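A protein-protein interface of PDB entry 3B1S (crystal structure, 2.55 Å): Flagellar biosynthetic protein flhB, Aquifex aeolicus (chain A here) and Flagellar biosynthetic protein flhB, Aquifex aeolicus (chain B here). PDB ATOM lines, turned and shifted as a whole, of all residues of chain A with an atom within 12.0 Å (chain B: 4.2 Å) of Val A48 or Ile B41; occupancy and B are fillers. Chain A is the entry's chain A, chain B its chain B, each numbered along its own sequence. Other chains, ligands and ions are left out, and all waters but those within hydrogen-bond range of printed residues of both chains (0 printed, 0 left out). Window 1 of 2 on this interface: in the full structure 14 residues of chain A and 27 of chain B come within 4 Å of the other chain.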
ATOM      1  N   MET A  39      -2.213 -31.841 -19.741  1.00  0.00           N
ATOM      2  CA  MET A  39      -2.313 -30.649 -20.527  1.00  0.00           C
ATOM      3  C   MET A  39      -2.996 -29.459 -19.788  1.00  0.00           C
ATOM      4  O   MET A  39      -2.432 -28.354 -19.762  1.00  0.00           O
ATOM      5  CB  MET A  39      -2.985 -30.985 -21.830  1.00  0.00           C
ATOM      6  CG  MET A  39      -3.205 -29.801 -22.650  1.00  0.00           C
ATOM      7  SD  MET A  39      -3.994 -30.182 -24.220  1.00  0.00           S
ATOM      8  CE  MET A  39      -5.713 -30.024 -23.755  1.00  0.00           C
ATOM      9  N   MET A  40      -4.165 -29.694 -19.166  1.00  0.00           N
ATOM     10  CA  MET A  40      -4.898 -28.662 -18.395  1.00  0.00           C
ATOM     11  C   MET A  40      -4.202 -28.196 -17.155  1.00  0.00           C
ATOM     12  O   MET A  40      -4.511 -27.149 -16.624  1.00  0.00           O
ATOM     13  CB  MET A  40      -6.275 -29.140 -17.978  1.00  0.00           C
ATOM     14  CG  MET A  40      -7.137 -29.527 -19.136  1.00  0.00           C
ATOM     15  SD  MET A  40      -7.465 -28.114 -20.190  1.00  0.00           S
ATOM     16  CE  MET A  40      -7.965 -28.985 -21.658  1.00  0.00           C
ATOM     17  N   ALA A  41      -3.287 -28.992 -16.660  1.00  0.00           N
ATOM     18  CA  ALA A  41      -2.522 -28.594 -15.501  1.00  0.00           C
ATOM     19  C   ALA A  41      -1.327 -27.706 -15.938  1.00  0.00           C
ATOM     20  O   ALA A  41      -0.773 -26.921 -15.138  1.00  0.00           O
ATOM     21  CB  ALA A  41      -2.044 -29.850 -14.763  1.00  0.00           C
ATOM     22  N   GLU A  42      -0.930 -27.843 -17.208  1.00  0.00           N
ATOM     23  CA  GLU A  42       0.200 -27.088 -17.749  1.00  0.00           C
ATOM     24  C   GLU A  42      -0.215 -25.695 -18.251  1.00  0.00           C
ATOM     25  O   GLU A  42       0.643 -24.877 -18.624  1.00  0.00           O
ATOM     26  CB  GLU A  42       0.909 -27.889 -18.859  1.00  0.00           C
ATOM     27  CG  GLU A  42       1.973 -28.869 -18.347  1.00  0.00           C
ATOM     28  CD  GLU A  42       3.068 -28.200 -17.472  1.00  0.00           C
ATOM     29  OE1 GLU A  42       3.008 -28.347 -16.228  1.00  0.00           O
ATOM     30  OE2 GLU A  42       3.982 -27.531 -18.018  1.00  0.00           O
ATOM     31  N   VAL A  43      -1.530 -25.446 -18.276  1.00  0.00           N
ATOM     32  CA  VAL A  43      -2.093 -24.160 -18.701  1.00  0.00           C
ATOM     33  C   VAL A  43      -1.763 -22.987 -17.755  1.00  0.00           C
ATOM     34  O   VAL A  43      -1.542 -21.883 -18.242  1.00  0.00           O
ATOM     35  CB  VAL A  43      -3.616 -24.245 -18.954  1.00  0.00           C
ATOM     36  CG1 VAL A  43      -4.198 -22.858 -19.127  1.00  0.00           C
ATOM     37  CG2 VAL A  43      -3.921 -25.142 -20.171  1.00  0.00           C
ATOM     38  N   PRO A  44      -1.562 -23.225 -16.485  1.00  0.00           N
ATOM     39  CA  PRO A  44      -1.258 -22.151 -15.561  1.00  0.00           C
ATOM     40  C   PRO A  44       0.097 -21.567 -15.854  1.00  0.00           C
ATOM     41  O   PRO A  44       0.539 -20.635 -15.229  1.00  0.00           O
ATOM     42  CB  PRO A  44      -1.271 -22.867 -14.237  1.00  0.00           C
ATOM     43  CG  PRO A  44      -2.360 -23.770 -14.400  1.00  0.00           C
ATOM     44  CD  PRO A  44      -2.336 -24.258 -15.809  1.00  0.00           C
ATOM     45  N   LYS A  45       0.782 -22.197 -16.778  1.00  0.00           N
ATOM     46  CA  LYS A  45       2.131 -21.834 -17.153  1.00  0.00           C
ATOM     47  C   LYS A  45       2.106 -21.103 -18.487  1.00  0.00           C
ATOM     48  O   LYS A  45       3.146 -20.740 -18.995  1.00  0.00           O
ATOM     49  CB  LYS A  45       3.023 -23.088 -17.253  1.00  0.00           C
ATOM     50  CG  LYS A  45       3.116 -23.918 -15.968  1.00  0.00           C
ATOM     51  CD  LYS A  45       4.341 -24.838 -15.964  1.00  0.00           C
ATOM     52  CE  LYS A  45       4.352 -25.732 -14.707  1.00  0.00           C
ATOM     53  NZ  LYS A  45       4.966 -27.089 -14.918  1.00  0.00           N
ATOM     54  N   ALA A  46       0.946 -20.897 -19.062  1.00  0.00           N
ATOM     55  CA  ALA A  46       0.894 -20.228 -20.335  1.00  0.00           C
ATOM     56  C   ALA A  46       1.121 -18.752 -20.177  1.00  0.00           C
ATOM     57  O   ALA A  46       1.069 -18.243 -19.086  1.00  0.00           O
ATOM     58  CB  ALA A  46      -0.400 -20.494 -21.006  1.00  0.00           C
ATOM     59  N   THR A  47       1.406 -18.080 -21.280  1.00  0.00           N
ATOM     60  CA  THR A  47       1.612 -16.645 -21.293  1.00  0.00           C
ATOM     61  C   THR A  47       0.552 -16.044 -22.265  1.00  0.00           C
ATOM     62  O   THR A  47       0.261 -14.839 -22.231  1.00  0.00           O
ATOM     63  CB  THR A  47       3.049 -16.284 -21.804  1.00  0.00           C
ATOM     64  OG1 THR A  47       3.225 -16.821 -23.120  1.00  0.00           O
ATOM     65  CG2 THR A  47       4.123 -16.833 -20.932  1.00  0.00           C
ATOM     66  N   VAL A  48      -0.038 -16.875 -23.125  1.00  0.00           N
ATOM     67  CA  VAL A  48      -0.961 -16.374 -24.162  1.00  0.00           C
ATOM     68  C   VAL A  48      -1.837 -17.496 -24.667  1.00  0.00           C
ATOM     69  O   VAL A  48      -1.366 -18.629 -24.801  1.00  0.00           O
ATOM     70  CB  VAL A  48      -0.236 -15.874 -25.416  1.00  0.00           C
ATOM     71  CG1 VAL A  48      -1.156 -14.998 -26.199  1.00  0.00           C
ATOM     72  CG2 VAL A  48       1.082 -15.133 -25.053  1.00  0.00           C
ATOM     73  N   VAL A  49      -3.089 -17.184 -24.994  1.00  0.00           N
ATOM     74  CA  VAL A  49      -3.969 -18.164 -25.584  1.00  0.00           C
ATOM     75  C   VAL A  49      -4.564 -17.570 -26.798  1.00  0.00           C
ATOM     76  O   VAL A  49      -5.071 -16.475 -26.727  1.00  0.00           O
ATOM     77  CB  VAL A  49      -5.128 -18.508 -24.653  1.00  0.00           C
ATOM     78  CG1 VAL A  49      -6.031 -19.491 -25.324  1.00  0.00           C
ATOM     79  CG2 VAL A  49      -4.613 -19.054 -23.309  1.00  0.00           C
ATOM     80  N   ILE A  50      -4.546 -18.295 -27.900  1.00  0.00           N
ATOM     81  CA  ILE A  50      -5.242 -17.848 -29.070  1.00  0.00           C
ATOM     82  C   ILE A  50      -6.546 -18.571 -29.142  1.00  0.00           C
ATOM     83  O   ILE A  50      -6.602 -19.768 -28.901  1.00  0.00           O
ATOM     84  CB  ILE A  50      -4.426 -18.087 -30.307  1.00  0.00           C
ATOM     85  CG1 ILE A  50      -3.089 -17.310 -30.179  1.00  0.00           C
ATOM     86  CG2 ILE A  50      -5.230 -17.644 -31.577  1.00  0.00           C
ATOM     87  CD1 ILE A  50      -2.037 -17.679 -31.186  1.00  0.00           C
ATOM     88  N   THR A  51      -7.599 -17.830 -29.489  1.00  0.00           N
ATOM     89  CA  THR A  51      -9.005 -18.266 -29.425  1.00  0.00           C
ATOM     90  C   THR A  51      -9.641 -18.005 -30.773  1.00  0.00           C
ATOM     91  O   THR A  51      -9.177 -17.138 -31.507  1.00  0.00           O
ATOM     92  CB  THR A  51      -9.739 -17.422 -28.318  1.00  0.00           C
ATOM     93  OG1 THR A  51      -9.424 -17.959 -27.025  1.00  0.00           O
ATOM     94  CG2 THR A  51     -11.278 -17.339 -28.502  1.00  0.00           C
ATOM     95  N   ASN A  52     -10.711 -18.731 -31.093  1.00  0.00           N
ATOM     96  CA  ASN A  52     -11.531 -18.411 -32.281  1.00  0.00           C
ATOM     97  C   ASN A  52     -12.351 -17.111 -32.159  1.00  0.00           C
ATOM     98  O   ASN A  52     -12.908 -16.785 -31.088  1.00  0.00           O
ATOM     99  CB  ASN A  52     -12.419 -19.595 -32.724  1.00  0.00           C
ATOM    100  CG  ASN A  52     -13.760 -19.698 -31.943  1.00  0.00           C
ATOM    101  OD1 ASN A  52     -13.821 -19.514 -30.718  1.00  0.00           O
ATOM    102  ND2 ASN A  52     -14.829 -20.029 -32.668  1.00  0.00           N
ATOM    103  OXT ASN A  52     -12.470 -16.347 -33.141  1.00  0.00           O
ATOM    104  N   ILE B   6      -5.686 -22.276 -28.350  1.00  0.00           N
ATOM    105  CA  ILE B   6      -4.275 -22.755 -28.375  1.00  0.00           C
ATOM    106  C   ILE B   6      -3.414 -22.059 -27.344  1.00  0.00           C
ATOM    107  O   ILE B   6      -3.090 -20.923 -27.524  1.00  0.00           O
ATOM    108  CB  ILE B   6      -3.597 -22.533 -29.747  1.00  0.00           C
ATOM    109  CG1 ILE B   6      -4.579 -22.742 -30.897  1.00  0.00           C
ATOM    110  CG2 ILE B   6      -2.408 -23.417 -29.882  1.00  0.00           C
ATOM    111  CD1 ILE B   6      -5.233 -24.066 -30.912  1.00  0.00           C
ATOM    112  N   ALA B   7      -3.032 -22.739 -26.285  1.00  0.00           N
ATOM    113  CA  ALA B   7      -2.243 -22.107 -25.246  1.00  0.00           C
ATOM    114  C   ALA B   7      -0.720 -22.134 -25.538  1.00  0.00           C
ATOM    115  O   ALA B   7      -0.188 -23.128 -26.025  1.00  0.00           O
ATOM    116  CB  ALA B   7      -2.538 -22.730 -23.935  1.00  0.00           C
ATOM    117  N   LEU B   8      -0.026 -21.027 -25.248  1.00  0.00           N
ATOM    118  CA  LEU B   8       1.376 -20.878 -25.611  1.00  0.00           C
ATOM    119  C   LEU B   8       2.157 -20.371 -24.433  1.00  0.00           C
ATOM    120  O   LEU B   8       1.687 -19.505 -23.708  1.00  0.00           O
ATOM    121  CB  LEU B   8       1.550 -19.960 -26.825  1.00  0.00           C
ATOM    122  CG  LEU B   8       0.899 -20.416 -28.152  1.00  0.00           C
ATOM    123  CD1 LEU B   8       1.185 -19.444 -29.304  1.00  0.00           C
ATOM    124  CD2 LEU B   8       1.289 -21.811 -28.581  1.00  0.00           C
ATOM    125  N   ALA B  36      -7.009 -19.994 -17.653  1.00  0.00           N
ATOM    126  CA  ALA B  36      -6.174 -18.880 -17.983  1.00  0.00           C
ATOM    127  C   ALA B  36      -6.787 -17.612 -17.475  1.00  0.00           C
ATOM    128  O   ALA B  36      -6.160 -16.884 -16.748  1.00  0.00           O
ATOM    129  CB  ALA B  36      -6.003 -18.802 -19.454  1.00  0.00           C
ATOM    130  N   TYR B  39      -5.861 -17.429 -14.269  1.00  0.00           N
ATOM    131  CA  TYR B  39      -4.514 -16.991 -13.890  1.00  0.00           C
ATOM    132  C   TYR B  39      -4.095 -15.582 -14.376  1.00  0.00           C
ATOM    133  O   TYR B  39      -2.943 -15.176 -14.213  1.00  0.00           O
ATOM    134  CB  TYR B  39      -3.511 -18.062 -14.325  1.00  0.00           C
ATOM    135  CG  TYR B  39      -3.485 -19.203 -13.357  1.00  0.00           C
ATOM    136  CD1 TYR B  39      -2.448 -19.319 -12.437  1.00  0.00           C
ATOM    137  CD2 TYR B  39      -4.525 -20.130 -13.318  1.00  0.00           C
ATOM    138  CE1 TYR B  39      -2.425 -20.344 -11.528  1.00  0.00           C
ATOM    139  CE2 TYR B  39      -4.522 -21.142 -12.411  1.00  0.00           C
ATOM    140  CZ  TYR B  39      -3.466 -21.250 -11.520  1.00  0.00           C
ATOM    141  OH  TYR B  39      -3.450 -22.281 -10.616  1.00  0.00           O
ATOM    142  N   SER B  40      -5.044 -14.855 -14.966  1.00  0.00           N
ATOM    143  CA  SER B  40      -4.809 -13.543 -15.575  1.00  0.00           C
ATOM    144  C   SER B  40      -3.846 -13.631 -16.769  1.00  0.00           C
ATOM    145  O   SER B  40      -3.094 -12.686 -17.078  1.00  0.00           O
ATOM    146  CB  SER B  40      -4.336 -12.529 -14.524  1.00  0.00           C
ATOM    147  OG  SER B  40      -5.230 -12.515 -13.416  1.00  0.00           O
ATOM    148  N   ILE B  41      -3.884 -14.782 -17.428  1.00  0.00           N
ATOM    149  CA  ILE B  41      -3.176 -15.011 -18.664  1.00  0.00           C
ATOM    150  C   ILE B  41      -4.077 -14.458 -19.787  1.00  0.00           C
ATOM    151  O   ILE B  41      -5.233 -14.868 -19.929  1.00  0.00           O
ATOM    152  CB  ILE B  41      -2.805 -16.545 -18.799  1.00  0.00           C
ATOM    153  CG1 ILE B  41      -1.715 -16.916 -17.773  1.00  0.00           C
ATOM    154  CG2 ILE B  41      -2.370 -16.904 -20.188  1.00  0.00           C
ATOM    155  CD1 ILE B  41      -1.826 -18.309 -17.174  1.00  0.00           C
ATOM    156  N   PRO B  42      -3.492 -13.661 -20.656  1.00  0.00           N
ATOM    157  CA  PRO B  42      -4.178 -12.976 -21.736  1.00  0.00           C
ATOM    158  C   PRO B  42      -4.755 -13.931 -22.709  1.00  0.00           C
ATOM    159  O   PRO B  42      -4.339 -15.047 -22.781  1.00  0.00           O
ATOM    160  CB  PRO B  42      -3.053 -12.247 -22.413  1.00  0.00           C
ATOM    161  CG  PRO B  42      -2.125 -11.948 -21.347  1.00  0.00           C
ATOM    162  CD  PRO B  42      -2.288 -12.935 -20.256  1.00  0.00           C
ATOM    163  N   VAL B  43      -5.758 -13.487 -23.426  1.00  0.00           N
ATOM    164  CA  VAL B  43      -6.528 -14.355 -24.260  1.00  0.00           C
ATOM    165  C   VAL B  43      -6.899 -13.560 -25.496  1.00  0.00           C
ATOM    166  O   VAL B  43      -7.528 -12.519 -25.425  1.00  0.00           O
ATOM    167  CB  VAL B  43      -7.819 -14.820 -23.516  1.00  0.00           C
ATOM    168  CG1 VAL B  43      -8.684 -15.739 -24.392  1.00  0.00           C
ATOM    169  CG2 VAL B  43      -7.482 -15.478 -22.178  1.00  0.00           C
ATOM    170  N   ILE B  74       1.158 -11.179 -32.205  1.00  0.00           N
ATOM    171  CA  ILE B  74       0.287 -11.268 -31.054  1.00  0.00           C
ATOM    172  C   ILE B  74       0.990 -11.088 -29.727  1.00  0.00           C
ATOM    173  O   ILE B  74       0.642 -10.217 -28.973  1.00  0.00           O
ATOM    174  CB  ILE B  74      -0.400 -12.631 -31.029  1.00  0.00           C
ATOM    175  CG1 ILE B  74      -1.439 -12.703 -32.125  1.00  0.00           C
ATOM    176  CG2 ILE B  74      -1.075 -12.881 -29.725  1.00  0.00           C
ATOM    177  CD1 ILE B  74      -2.101 -11.389 -32.388  1.00  0.00           C
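Among the printed residues, pairs that only touch across the chains: Val A43 with Ile B41 (3.7 Å), Pro A44 with Tyr B39 (3.8 Å), Pro A44 with Ile B41 (3.8 Å), Ala A46 with Leu B8 (3.5 Å), Ala A46 with Ile B41 (3.4 Å), Thr A47 with Ile B41 (3.7 Å), Thr A47 with Pro B42 (3.7 Å), Val A48 with Ile B6 (3.96 Å), Val A48 with Ala B7 (3.6 Å), Val A48 with Ile B41 (3.8 Å), Val A48 with Pro B42 (3.9 Å), Val A49 with Ile B6 (3.5 Å), Val A49 with Val B43 (3.6 Å) and Thr A51 with Val B43 (3.5 Å).
Printed residues of chain B that touch a printed residue of chain A: Ile B6, Ala B7, Leu B8, Tyr B39, Ile B41, Pro B42 and Val B43. Hydrophobic or aromatic side chains of chain B that line the printed part of chain A: Leu B8, Tyr B39, Ile B41, Pro B42 and Val B43. Among the printed residues, no Asp or Glu carboxylate lies within 4 Å of a Lys or Arg side-chain nitrogen of the other chain.
N of Ile B41 lies within hydrogen-bond range of O of Ala B36, at 3.2 Å.
Of the printed residues of chain B, Ala A46 touches Leu B8 (3.5 Å) and Ile B41 (3.4 Å). Val A48 touches just these residues of chain B: Ile B6 (3.96 Å), Ala B7 (3.6 Å), Leu B8 (2.8 Å), Ile B41 (3.8 Å) and Pro B42 (3.9 Å). Printed residues of chain B within 4 Å of Ile A50: Ile B6 (2.7 Å). Of the printed residues of chain B, Thr A51 touches Val B43. Asn A52 touches none of the printed residues of chain B. Of the printed residues of chain A, Ile B6 touches Val A48, Val A49 and Ile A50. Of chain A, only Val A48 comes within 4 Å of Ala B7. No residue of chain A comes within 4 Å of Ala B36. Of chain A, only Pro A44 comes within 4 Å of Tyr B39. No residue of chain A comes within 4 Å of Ser B40. Ile B41 touches five residues of chain A. Of the printed residues of chain A, Val B43 touches Val A49 (3.6 Å) and Thr A51 (3.5 Å). No residue of chain A comes within 4 Å of Ile B74. The nearest residue of chain B that does not touch Val A48 is Ile B74 (4.1 Å).
O of Val A48 lies within hydrogen-bond range of N of Leu B8 (2.8 Å). The backbone carbonyl oxygen (O) of Leu B8 lies within hydrogen-bond range of the backbone NH (N) of Thr A47 (2.8 Å). The backbone NH (N) of Val A49 lies within hydrogen-bond range of the backbone carbonyl oxygen (O) of Pro B42 (3.3 Å). The backbone carbonyl oxygen (O) of Ile A50 lies within hydrogen-bond range of the backbone NH (N) of Ile B6, 2.7 Å away.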
